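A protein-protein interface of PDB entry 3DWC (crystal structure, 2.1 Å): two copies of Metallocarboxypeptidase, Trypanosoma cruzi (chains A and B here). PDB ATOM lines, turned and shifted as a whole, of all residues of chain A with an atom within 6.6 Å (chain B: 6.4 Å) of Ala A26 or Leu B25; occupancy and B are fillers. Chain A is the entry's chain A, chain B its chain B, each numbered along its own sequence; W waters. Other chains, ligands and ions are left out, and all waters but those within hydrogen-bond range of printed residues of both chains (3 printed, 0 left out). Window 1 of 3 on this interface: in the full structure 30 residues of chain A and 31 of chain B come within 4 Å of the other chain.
Water W2 lies within hydrogen-bond range of the side-chain carboxylate (OD1) of Asp A29 (2.8 Å) and the side-chain carboxylate (OD1) of Asp B29 (2.8 Å). Water W1 lies within hydrogen-bond range of the guanidinium group (NH2) of Arg A42, the side-chain amide nitrogen (ND2) of Asn B242, the side-chain carboxylate (OD2) of Asp B246 and a ring nitrogen (NE2) of His B21. Water W3 lies within hydrogen-bond range of ND2 of Asn A242, NH2 of Arg B42 and NE2 of His A21.
The side-chain carboxylate (OD2) of Asp B29 is in salt-bridge range of the guanidinium group (NH1) of Arg B42, 3.0 Å away. The backbone carbonyl oxygen of Ala B26 lies within hydrogen-bond range of the guanidinium group of Arg B42, at 3.0 Å. The side-chain amide nitrogen of Asn B242 lies close to the guanidinium group of Arg B248, at 3.3 Å. The side-chain carboxylate (OD2) of Asp A29 is in salt-bridge range of the guanidinium group (NH1) of Arg A42 (2.9 Å). O of Ala A26 is in hydrogen-bond range of NH1 of Arg A42, at 3.0 Å. The side-chain carboxylate (OD1) of Asp B246 lies within salt-bridge range of the guanidinium group (NE) of Arg B248 (2.8 Å).
Met A22 touches Ala B26 (CE to CB, 3.7 Å). Ala B26 touches Leu A25. Leu A25 touches Asp B29. Met B22 touches Ala A26. Leu B25 touches Ala A26 (CD2 to CA, 3.7 Å). OD1 of Asp A29 touches CD1 of Leu B25, 3.7 Å away. Met A34 touches Asp B246 (CG to OD2, 3.5 Å). NH2 of Arg B248 touches CA of Met A34 (3.4 Å). NH2 of Arg A42 touches NH2 of Arg B248 (3.7 Å). Met B22 touches Met A46.
Of the 15 printed residues of chain A, 9 touch a printed residue of chain B. Printed residues of chain A that touch a printed residue of chain B: His A21, Met A22, Leu A25, Ala A26, Trp A28, Asp A29, Met A34, Arg A42 and Met A46. Hydrophobic or aromatic side chains of chain A that line the printed part of chain B: His A21, Met A22, Leu A25, Ala A26, Trp A28, Met A34 and Met A46. Among the printed residues, Asp or Glu carboxylates within 4 Å of a Lys or Arg side-chain nitrogen of the other chain: Asp A29 with Arg B248.
The guanidinium group (NE) of Arg A42 sits at hydrogen-bond distance from a ring nitrogen (NE2) of His B21, at 2.9 Å. NE of Arg B42 sits at hydrogen-bond distance from NE2 of His A21, at 3.0 Å. The side-chain carboxylate of Asp A29 is in salt-bridge range of the guanidinium group of Arg B248, 2.9 Å away.
Of the printed residues of chain B, Met A22 touches Met B22 (3.97 Å) and Ala B26 (3.7 Å). Leu A23 touches none of the printed residues of chain B. Ser A30 touches none of the printed residues of chain B. Leu B25 touches just these residues of chain A: Ala A26, Asp A29 and Arg A42. Printed residues of chain A within 4 Å of Ala B26: Met A22 and Leu A25. Of the printed residues of chain A, Arg B42 touches His A21 (3.0 Å) and Leu A25 (3.6 Å). The nearest residue of chain B that does not touch Ala A26 is His B21 (5.9 Å).
His A21 touches Arg B42, and with the chains exchanged Arg A42 touches His B21. Met B22 touches its own counterpart, Met A22. Leu A25 touches Ala B26, and with the chains exchanged Ala A26 touches Leu B25. Leu A25 touches Arg B42, and with the chains exchanged Arg A42 touches Leu B25. Positions printed for both chains: 21, 22, 23, 24, 25, 26, 27, 28, 29, 30, 42 and 242.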
ATOM      1  N   HIS A  21     -31.070 -20.554 -19.463  1.00  0.00           N
ATOM      2  CA  HIS A  21     -29.756 -20.260 -18.887  1.00  0.00           C
ATOM      3  C   HIS A  21     -29.873 -19.508 -17.553  1.00  0.00           C
ATOM      4  O   HIS A  21     -29.218 -19.846 -16.565  1.00  0.00           O
ATOM      5  CB  HIS A  21     -28.918 -19.472 -19.888  1.00  0.00           C
ATOM      6  CG  HIS A  21     -27.622 -18.955 -19.333  1.00  0.00           C
ATOM      7  ND1 HIS A  21     -26.400 -19.446 -19.731  1.00  0.00           N
ATOM      8  CD2 HIS A  21     -27.360 -17.965 -18.442  1.00  0.00           C
ATOM      9  CE1 HIS A  21     -25.441 -18.787 -19.104  1.00  0.00           C
ATOM     10  NE2 HIS A  21     -25.996 -17.904 -18.300  1.00  0.00           N
ATOM     11  N   MET A  22     -30.741 -18.508 -17.544  1.00  0.00           N
ATOM     12  CA  MET A  22     -30.937 -17.686 -16.377  1.00  0.00           C
ATOM     13  C   MET A  22     -31.562 -18.508 -15.264  1.00  0.00           C
ATOM     14  O   MET A  22     -31.149 -18.430 -14.117  1.00  0.00           O
ATOM     15  CB  MET A  22     -31.819 -16.487 -16.728  1.00  0.00           C
ATOM     16  CG  MET A  22     -31.143 -15.510 -17.691  1.00  0.00           C
ATOM     17  SD  MET A  22     -29.793 -14.706 -16.780  1.00  0.00           S
ATOM     18  CE  MET A  22     -29.140 -13.622 -17.967  1.00  0.00           C
ATOM     19  N   LEU A  23     -32.584 -19.275 -15.597  1.00  0.00           N
ATOM     20  CA  LEU A  23     -33.224 -20.150 -14.613  1.00  0.00           C
ATOM     21  C   LEU A  23     -32.319 -21.190 -14.021  1.00  0.00           C
ATOM     22  O   LEU A  23     -32.427 -21.476 -12.832  1.00  0.00           O
ATOM     23  CB  LEU A  23     -34.392 -20.924 -15.212  1.00  0.00           C
ATOM     24  CG  LEU A  23     -35.760 -20.342 -15.206  1.00  0.00           C
ATOM     25  CD1 LEU A  23     -36.713 -21.472 -15.758  1.00  0.00           C
ATOM     26  CD2 LEU A  23     -36.167 -19.883 -13.768  1.00  0.00           C
ATOM     27  N   LEU A  24     -31.483 -21.775 -14.854  1.00  0.00           N
ATOM     28  CA  LEU A  24     -30.494 -22.787 -14.459  1.00  0.00           C
ATOM     29  C   LEU A  24     -29.465 -22.201 -13.491  1.00  0.00           C
ATOM     30  O   LEU A  24     -29.210 -22.774 -12.364  1.00  0.00           O
ATOM     31  CB  LEU A  24     -29.850 -23.406 -15.714  1.00  0.00           C
ATOM     32  CG  LEU A  24     -30.805 -24.382 -16.490  1.00  0.00           C
ATOM     33  CD1 LEU A  24     -30.253 -24.809 -17.859  1.00  0.00           C
ATOM     34  CD2 LEU A  24     -31.073 -25.662 -15.677  1.00  0.00           C
ATOM     35  N   LEU A  25     -28.958 -21.009 -13.844  1.00  0.00           N
ATOM     36  CA  LEU A  25     -28.031 -20.299 -12.929  1.00  0.00           C
ATOM     37  C   LEU A  25     -28.719 -19.998 -11.600  1.00  0.00           C
ATOM     38  O   LEU A  25     -28.197 -20.295 -10.557  1.00  0.00           O
ATOM     39  CB  LEU A  25     -27.494 -19.018 -13.539  1.00  0.00           C
ATOM     40  CG  LEU A  25     -26.542 -18.260 -12.632  1.00  0.00           C
ATOM     41  CD1 LEU A  25     -25.279 -19.024 -12.487  1.00  0.00           C
ATOM     42  CD2 LEU A  25     -26.310 -16.828 -13.211  1.00  0.00           C
ATOM     43  N   ALA A  26     -29.910 -19.438 -11.639  1.00  0.00           N
ATOM     44  CA  ALA A  26     -30.678 -19.120 -10.419  1.00  0.00           C
ATOM     45  C   ALA A  26     -30.909 -20.349  -9.537  1.00  0.00           C
ATOM     46  O   ALA A  26     -30.853 -20.291  -8.280  1.00  0.00           O
ATOM     47  CB  ALA A  26     -32.007 -18.490 -10.815  1.00  0.00           C
ATOM     48  N   ASP A  27     -31.185 -21.478 -10.172  1.00  0.00           N
ATOM     49  CA  ASP A  27     -31.442 -22.692  -9.421  1.00  0.00           C
ATOM     50  C   ASP A  27     -30.146 -23.207  -8.744  1.00  0.00           C
ATOM     51  O   ASP A  27     -30.122 -23.494  -7.530  1.00  0.00           O
ATOM     52  CB  ASP A  27     -32.155 -23.738 -10.261  1.00  0.00           C
ATOM     53  CG  ASP A  27     -32.610 -24.907  -9.408  1.00  0.00           C
ATOM     54  OD1 ASP A  27     -33.379 -24.678  -8.408  1.00  0.00           O
ATOM     55  OD2 ASP A  27     -32.084 -25.988  -9.646  1.00  0.00           O
ATOM     56  N   TRP A  28     -29.048 -23.245  -9.478  1.00  0.00           N
ATOM     57  CA  TRP A  28     -27.774 -23.636  -8.916  1.00  0.00           C
ATOM     58  C   TRP A  28     -27.380 -22.742  -7.741  1.00  0.00           C
ATOM     59  O   TRP A  28     -26.939 -23.208  -6.721  1.00  0.00           O
ATOM     60  CB  TRP A  28     -26.701 -23.547 -10.004  1.00  0.00           C
ATOM     61  CG  TRP A  28     -25.319 -23.750  -9.485  1.00  0.00           C
ATOM     62  CD1 TRP A  28     -24.679 -24.932  -9.293  1.00  0.00           C
ATOM     63  CD2 TRP A  28     -24.434 -22.722  -9.027  1.00  0.00           C
ATOM     64  NE1 TRP A  28     -23.454 -24.710  -8.692  1.00  0.00           N
ATOM     65  CE2 TRP A  28     -23.274 -23.356  -8.539  1.00  0.00           C
ATOM     66  CE3 TRP A  28     -24.526 -21.322  -8.958  1.00  0.00           C
ATOM     67  CZ2 TRP A  28     -22.167 -22.631  -8.055  1.00  0.00           C
ATOM     68  CZ3 TRP A  28     -23.437 -20.589  -8.420  1.00  0.00           C
ATOM     69  CH2 TRP A  28     -22.265 -21.259  -8.002  1.00  0.00           C
ATOM     70  N   ASP A  29     -27.507 -21.441  -7.926  1.00  0.00           N
ATOM     71  CA  ASP A  29     -27.051 -20.487  -6.972  1.00  0.00           C
ATOM     72  C   ASP A  29     -27.875 -20.643  -5.687  1.00  0.00           C
ATOM     73  O   ASP A  29     -27.317 -20.600  -4.613  1.00  0.00           O
ATOM     74  CB  ASP A  29     -27.196 -19.084  -7.569  1.00  0.00           C
ATOM     75  CG  ASP A  29     -26.762 -18.014  -6.618  1.00  0.00           C
ATOM     76  OD1 ASP A  29     -25.596 -17.573  -6.729  1.00  0.00           O
ATOM     77  OD2 ASP A  29     -27.559 -17.664  -5.722  1.00  0.00           O
ATOM     78  N   SER A  30     -29.185 -20.871  -5.836  1.00  0.00           N
ATOM     79  CA  SER A  30     -30.130 -21.190  -4.720  1.00  0.00           C
ATOM     80  C   SER A  30     -29.637 -22.217  -3.749  1.00  0.00           C
ATOM     81  O   SER A  30     -29.882 -22.119  -2.549  1.00  0.00           O
ATOM     82  CB  SER A  30     -31.442 -21.754  -5.282  1.00  0.00           C
ATOM     83  OG  SER A  30     -32.154 -20.592  -5.612  1.00  0.00           O
ATOM     84  N   HIS A  31     -29.006 -23.232  -4.300  1.00  0.00           N
ATOM     85  CA  HIS A  31     -28.490 -24.338  -3.504  1.00  0.00           C
ATOM     86  C   HIS A  31     -27.047 -24.224  -3.068  1.00  0.00           C
ATOM     87  O   HIS A  31     -26.634 -24.988  -2.247  1.00  0.00           O
ATOM     88  CB  HIS A  31     -28.668 -25.642  -4.280  1.00  0.00           C
ATOM     89  CG  HIS A  31     -30.100 -25.950  -4.577  1.00  0.00           C
ATOM     90  ND1 HIS A  31     -30.632 -25.896  -5.846  1.00  0.00           N
ATOM     91  CD2 HIS A  31     -31.134 -26.239  -3.749  1.00  0.00           C
ATOM     92  CE1 HIS A  31     -31.923 -26.171  -5.793  1.00  0.00           C
ATOM     93  NE2 HIS A  31     -32.251 -26.383  -4.532  1.00  0.00           N
ATOM     94  N   MET A  34     -26.687 -18.740  -2.264  1.00  0.00           N
ATOM     95  CA  MET A  34     -27.673 -17.802  -1.802  1.00  0.00           C
ATOM     96  C   MET A  34     -27.835 -17.793  -0.293  1.00  0.00           C
ATOM     97  O   MET A  34     -28.099 -18.825   0.303  1.00  0.00           O
ATOM     98  CB  MET A  34     -29.017 -18.137  -2.428  1.00  0.00           C
ATOM     99  CG  MET A  34     -30.109 -17.105  -2.211  1.00  0.00           C
ATOM    100  SD  MET A  34     -31.690 -17.839  -2.717  1.00  0.00           S
ATOM    101  CE  MET A  34     -31.861 -19.174  -1.552  1.00  0.00           C
ATOM    102  N   ARG A  42     -35.696 -14.669  -4.726  1.00  0.00           N
ATOM    103  CA  ARG A  42     -35.209 -15.614  -5.727  1.00  0.00           C
ATOM    104  C   ARG A  42     -36.367 -16.462  -6.254  1.00  0.00           C
ATOM    105  O   ARG A  42     -36.471 -16.681  -7.426  1.00  0.00           O
ATOM    106  CB  ARG A  42     -34.157 -16.523  -5.115  1.00  0.00           C
ATOM    107  CG  ARG A  42     -33.660 -17.667  -6.038  1.00  0.00           C
ATOM    108  CD  ARG A  42     -33.003 -17.151  -7.321  1.00  0.00           C
ATOM    109  NE  ARG A  42     -31.912 -16.247  -6.993  1.00  0.00           N
ATOM    110  CZ  ARG A  42     -30.676 -16.624  -6.659  1.00  0.00           C
ATOM    111  NH1 ARG A  42     -30.341 -17.903  -6.584  1.00  0.00           N
ATOM    112  NH2 ARG A  42     -29.785 -15.707  -6.334  1.00  0.00           N
ATOM    113  N   MET A  46     -37.670 -16.524 -10.203  1.00  0.00           N
ATOM    114  CA  MET A  46     -37.643 -17.718 -11.010  1.00  0.00           C
ATOM    115  C   MET A  46     -39.047 -17.991 -11.561  1.00  0.00           C
ATOM    116  O   MET A  46     -39.197 -18.349 -12.714  1.00  0.00           O
ATOM    117  CB  MET A  46     -37.128 -18.917 -10.213  1.00  0.00           C
ATOM    118  CG  MET A  46     -35.729 -18.742  -9.754  1.00  0.00           C
ATOM    119  SD  MET A  46     -35.091 -20.129  -8.829  1.00  0.00           S
ATOM    120  CE  MET A  46     -35.013 -21.377 -10.130  1.00  0.00           C
ATOM    121  N   ASN A 242     -26.647 -26.282 -13.722  1.00  0.00           N
ATOM    122  CA  ASN A 242     -26.295 -25.126 -14.529  1.00  0.00           C
ATOM    123  C   ASN A 242     -26.367 -25.525 -16.005  1.00  0.00           C
ATOM    124  O   ASN A 242     -27.217 -26.327 -16.364  1.00  0.00           O
ATOM    125  CB  ASN A 242     -24.982 -24.416 -14.052  1.00  0.00           C
ATOM    126  CG  ASN A 242     -24.943 -22.950 -14.468  1.00  0.00           C
ATOM    127  OD1 ASN A 242     -25.982 -22.284 -14.476  1.00  0.00           O
ATOM    128  ND2 ASN A 242     -23.783 -22.466 -14.919  1.00  0.00           N
ATOM    129  N   GLY B  20     -34.998  -8.147 -13.493  1.00  0.00           N
ATOM    130  CA  GLY B  20     -33.756  -7.471 -13.084  1.00  0.00           C
ATOM    131  C   GLY B  20     -32.975  -8.274 -12.073  1.00  0.00           C
ATOM    132  O   GLY B  20     -31.743  -8.327 -12.122  1.00  0.00           O
ATOM    133  N   HIS B  21     -33.697  -8.944 -11.174  1.00  0.00           N
ATOM    134  CA  HIS B  21     -33.080  -9.926 -10.281  1.00  0.00           C
ATOM    135  C   HIS B  21     -32.173 -10.926 -11.020  1.00  0.00           C
ATOM    136  O   HIS B  21     -31.011 -11.096 -10.666  1.00  0.00           O
ATOM    137  CB  HIS B  21     -34.151 -10.639  -9.517  1.00  0.00           C
ATOM    138  CG  HIS B  21     -33.650 -11.721  -8.616  1.00  0.00           C
ATOM    139  ND1 HIS B  21     -33.541 -11.563  -7.241  1.00  0.00           N
ATOM    140  CD2 HIS B  21     -33.318 -13.010  -8.879  1.00  0.00           C
ATOM    141  CE1 HIS B  21     -33.127 -12.704  -6.713  1.00  0.00           C
ATOM    142  NE2 HIS B  21     -32.980 -13.594  -7.682  1.00  0.00           N
ATOM    143  N   MET B  22     -32.705 -11.572 -12.044  1.00  0.00           N
ATOM    144  CA  MET B  22     -31.903 -12.465 -12.913  1.00  0.00           C
ATOM    145  C   MET B  22     -30.652 -11.840 -13.513  1.00  0.00           C
ATOM    146  O   MET B  22     -29.570 -12.417 -13.466  1.00  0.00           O
ATOM    147  CB  MET B  22     -32.789 -12.994 -14.024  1.00  0.00           C
ATOM    148  CG  MET B  22     -33.945 -13.889 -13.508  1.00  0.00           C
ATOM    149  SD  MET B  22     -33.270 -15.389 -12.706  1.00  0.00           S
ATOM    150  CE  MET B  22     -34.706 -16.244 -12.183  1.00  0.00           C
ATOM    151  N   LEU B  23     -30.799 -10.650 -14.079  1.00  0.00           N
ATOM    152  CA  LEU B  23     -29.688  -9.925 -14.680  1.00  0.00           C
ATOM    153  C   LEU B  23     -28.590  -9.586 -13.676  1.00  0.00           C
ATOM    154  O   LEU B  23     -27.415  -9.742 -13.943  1.00  0.00           O
ATOM    155  CB  LEU B  23     -30.195  -8.602 -15.278  1.00  0.00           C
ATOM    156  CG  LEU B  23     -30.752  -8.633 -16.689  1.00  0.00           C
ATOM    157  CD1 LEU B  23     -30.991  -7.190 -17.160  1.00  0.00           C
ATOM    158  CD2 LEU B  23     -29.785  -9.361 -17.594  1.00  0.00           C
ATOM    159  N   LEU B  24     -28.999  -9.122 -12.518  1.00  0.00           N
ATOM    160  CA  LEU B  24     -28.049  -8.752 -11.467  1.00  0.00           C
ATOM    161  C   LEU B  24     -27.257  -9.985 -10.962  1.00  0.00           C
ATOM    162  O   LEU B  24     -26.046  -9.942 -10.698  1.00  0.00           O
ATOM    163  CB  LEU B  24     -28.844  -8.088 -10.349  1.00  0.00           C
ATOM    164  CG  LEU B  24     -29.383  -6.681 -10.639  1.00  0.00           C
ATOM    165  CD1 LEU B  24     -30.486  -6.262  -9.663  1.00  0.00           C
ATOM    166  CD2 LEU B  24     -28.233  -5.673 -10.576  1.00  0.00           C
ATOM    167  N   LEU B  25     -27.948 -11.107 -10.848  1.00  0.00           N
ATOM    168  CA  LEU B  25     -27.309 -12.381 -10.440  1.00  0.00           C
ATOM    169  C   LEU B  25     -26.343 -12.781 -11.484  1.00  0.00           C
ATOM    170  O   LEU B  25     -25.188 -13.092 -11.182  1.00  0.00           O
ATOM    171  CB  LEU B  25     -28.330 -13.497 -10.288  1.00  0.00           C
ATOM    172  CG  LEU B  25     -27.763 -14.830  -9.736  1.00  0.00           C
ATOM    173  CD1 LEU B  25     -27.225 -14.600  -8.275  1.00  0.00           C
ATOM    174  CD2 LEU B  25     -28.854 -15.943  -9.756  1.00  0.00           C
ATOM    175  N   ALA B  26     -26.814 -12.781 -12.727  1.00  0.00           N
ATOM    176  CA  ALA B  26     -25.976 -13.154 -13.888  1.00  0.00           C
ATOM    177  C   ALA B  26     -24.731 -12.276 -13.975  1.00  0.00           C
ATOM    178  O   ALA B  26     -23.656 -12.753 -14.303  1.00  0.00           O
ATOM    179  CB  ALA B  26     -26.792 -13.057 -15.195  1.00  0.00           C
ATOM    180  N   ASP B  27     -24.872 -10.998 -13.641  1.00  0.00           N
ATOM    181  CA  ASP B  27     -23.734 -10.067 -13.716  1.00  0.00           C
ATOM    182  C   ASP B  27     -22.788 -10.345 -12.559  1.00  0.00           C
ATOM    183  O   ASP B  27     -21.610 -10.471 -12.757  1.00  0.00           O
ATOM    184  CB  ASP B  27     -24.199  -8.620 -13.740  1.00  0.00           C
ATOM    185  CG  ASP B  27     -23.054  -7.652 -13.984  1.00  0.00           C
ATOM    186  OD1 ASP B  27     -22.393  -7.757 -15.048  1.00  0.00           O
ATOM    187  OD2 ASP B  27     -22.763  -6.867 -13.095  1.00  0.00           O
ATOM    188  N   TRP B  28     -23.321 -10.489 -11.349  1.00  0.00           N
ATOM    189  CA  TRP B  28     -22.499 -10.845 -10.202  1.00  0.00           C
ATOM    190  C   TRP B  28     -21.667 -12.106 -10.458  1.00  0.00           C
ATOM    191  O   TRP B  28     -20.434 -12.123 -10.245  1.00  0.00           O
ATOM    192  CB  TRP B  28     -23.371 -10.956  -8.905  1.00  0.00           C
ATOM    193  CG  TRP B  28     -22.595 -11.496  -7.749  1.00  0.00           C
ATOM    194  CD1 TRP B  28     -21.852 -10.788  -6.871  1.00  0.00           C
ATOM    195  CD2 TRP B  28     -22.444 -12.885  -7.388  1.00  0.00           C
ATOM    196  NE1 TRP B  28     -21.217 -11.643  -5.982  1.00  0.00           N
ATOM    197  CE2 TRP B  28     -21.553 -12.940  -6.298  1.00  0.00           C
ATOM    198  CE3 TRP B  28     -22.891 -14.085  -7.948  1.00  0.00           C
ATOM    199  CZ2 TRP B  28     -21.180 -14.150  -5.686  1.00  0.00           C
ATOM    200  CZ3 TRP B  28     -22.489 -15.304  -7.354  1.00  0.00           C
ATOM    201  CH2 TRP B  28     -21.637 -15.319  -6.236  1.00  0.00           C
ATOM    202  N   ASP B  29     -22.314 -13.144 -10.999  1.00  0.00           N
ATOM    203  CA  ASP B  29     -21.696 -14.431 -11.190  1.00  0.00           C
ATOM    204  C   ASP B  29     -20.638 -14.370 -12.263  1.00  0.00           C
ATOM    205  O   ASP B  29     -19.603 -15.078 -12.165  1.00  0.00           O
ATOM    206  CB  ASP B  29     -22.813 -15.448 -11.516  1.00  0.00           C
ATOM    207  CG  ASP B  29     -22.310 -16.823 -11.731  1.00  0.00           C
ATOM    208  OD1 ASP B  29     -22.363 -17.628 -10.793  1.00  0.00           O
ATOM    209  OD2 ASP B  29     -21.810 -17.120 -12.826  1.00  0.00           O
ATOM    210  N   SER B  30     -20.873 -13.575 -13.314  1.00  0.00           N
ATOM    211  CA  SER B  30     -19.898 -13.485 -14.407  1.00  0.00           C
ATOM    212  C   SER B  30     -18.548 -12.964 -13.888  1.00  0.00           C
ATOM    213  O   SER B  30     -17.528 -13.267 -14.452  1.00  0.00           O
ATOM    214  CB  SER B  30     -20.392 -12.598 -15.569  1.00  0.00           C
ATOM    215  OG  SER B  30     -20.534 -11.278 -15.078  1.00  0.00           O
ATOM    216  N   ARG B  42     -23.315 -16.750 -21.314  1.00  0.00           N
ATOM    217  CA  ARG B  42     -23.799 -15.793 -20.342  1.00  0.00           C
ATOM    218  C   ARG B  42     -24.148 -14.438 -20.978  1.00  0.00           C
ATOM    219  O   ARG B  42     -25.145 -13.834 -20.601  1.00  0.00           O
ATOM    220  CB  ARG B  42     -22.788 -15.610 -19.182  1.00  0.00           C
ATOM    221  CG  ARG B  42     -23.034 -14.529 -18.239  1.00  0.00           C
ATOM    222  CD  ARG B  42     -24.249 -14.743 -17.325  1.00  0.00           C
ATOM    223  NE  ARG B  42     -24.210 -16.092 -16.751  1.00  0.00           N
ATOM    224  CZ  ARG B  42     -23.435 -16.415 -15.718  1.00  0.00           C
ATOM    225  NH1 ARG B  42     -22.733 -15.475 -15.108  1.00  0.00           N
ATOM    226  NH2 ARG B  42     -23.383 -17.674 -15.282  1.00  0.00           N
ATOM    227  N   ASN B 242     -25.490  -7.558  -7.106  1.00  0.00           N
ATOM    228  CA  ASN B 242     -26.671  -8.341  -6.930  1.00  0.00           C
ATOM    229  C   ASN B 242     -27.877  -7.509  -6.491  1.00  0.00           C
ATOM    230  O   ASN B 242     -28.035  -6.406  -6.967  1.00  0.00           O
ATOM    231  CB  ASN B 242     -26.412  -9.525  -6.006  1.00  0.00           C
ATOM    232  CG  ASN B 242     -27.242 -10.713  -6.378  1.00  0.00           C
ATOM    233  OD1 ASN B 242     -27.518 -10.932  -7.552  1.00  0.00           O
ATOM    234  ND2 ASN B 242     -27.654 -11.484  -5.393  1.00  0.00           N
ATOM    235  N   SER B 243     -28.730  -8.033  -5.604  1.00  0.00           N
ATOM    236  CA  SER B 243     -30.030  -7.462  -5.328  1.00  0.00           C
ATOM    237  C   SER B 243     -30.173  -7.032  -3.863  1.00  0.00           C
ATOM    238  O   SER B 243     -29.400  -7.453  -2.985  1.00  0.00           O
ATOM    239  CB  SER B 243     -31.086  -8.516  -5.656  1.00  0.00           C
ATOM    240  OG  SER B 243     -31.167  -8.749  -7.054  1.00  0.00           O
ATOM    241  N   ASP B 246     -30.213  -9.516  -1.184  1.00  0.00           N
ATOM    242  CA  ASP B 246     -29.142 -10.462  -1.312  1.00  0.00           C
ATOM    243  C   ASP B 246     -27.983  -9.676  -1.890  1.00  0.00           C
ATOM    244  O   ASP B 246     -27.680  -9.790  -3.067  1.00  0.00           O
ATOM    245  CB  ASP B 246     -29.627 -11.623  -2.227  1.00  0.00           C
ATOM    246  CG  ASP B 246     -28.617 -12.752  -2.348  1.00  0.00           C
ATOM    247  OD1 ASP B 246     -27.418 -12.531  -1.991  1.00  0.00           O
ATOM    248  OD2 ASP B 246     -29.023 -13.858  -2.847  1.00  0.00           O
ATOM    249  N   ARG B 248     -24.262  -8.552  -2.526  1.00  0.00           N
ATOM    250  CA  ARG B 248     -23.052  -9.308  -2.676  1.00  0.00           C
ATOM    251  C   ARG B 248     -21.932  -8.340  -3.110  1.00  0.00           C
ATOM    252  O   ARG B 248     -21.977  -7.767  -4.202  1.00  0.00           O
ATOM    253  CB  ARG B 248     -23.233 -10.440  -3.717  1.00  0.00           C
ATOM    254  CG  ARG B 248     -24.363 -11.387  -3.332  1.00  0.00           C
ATOM    255  CD  ARG B 248     -24.383 -12.651  -4.153  1.00  0.00           C
ATOM    256  NE  ARG B 248     -25.520 -13.483  -3.767  1.00  0.00           N
ATOM    257  CZ  ARG B 248     -25.783 -14.648  -4.332  1.00  0.00           C
ATOM    258  NH1 ARG B 248     -24.998 -15.097  -5.279  1.00  0.00           N
ATOM    259  NH2 ARG B 248     -26.876 -15.317  -4.015  1.00  0.00           N
HETATM  260  O   HOH W   1     -30.170 -12.972  -5.790  1.00  0.00           O
HETATM  261  O   HOH W   2     -24.798 -17.379  -9.356  1.00  0.00           O
HETATM  262  O   HOH W   3     -24.156 -20.176 -16.554  1.00  0.00           O
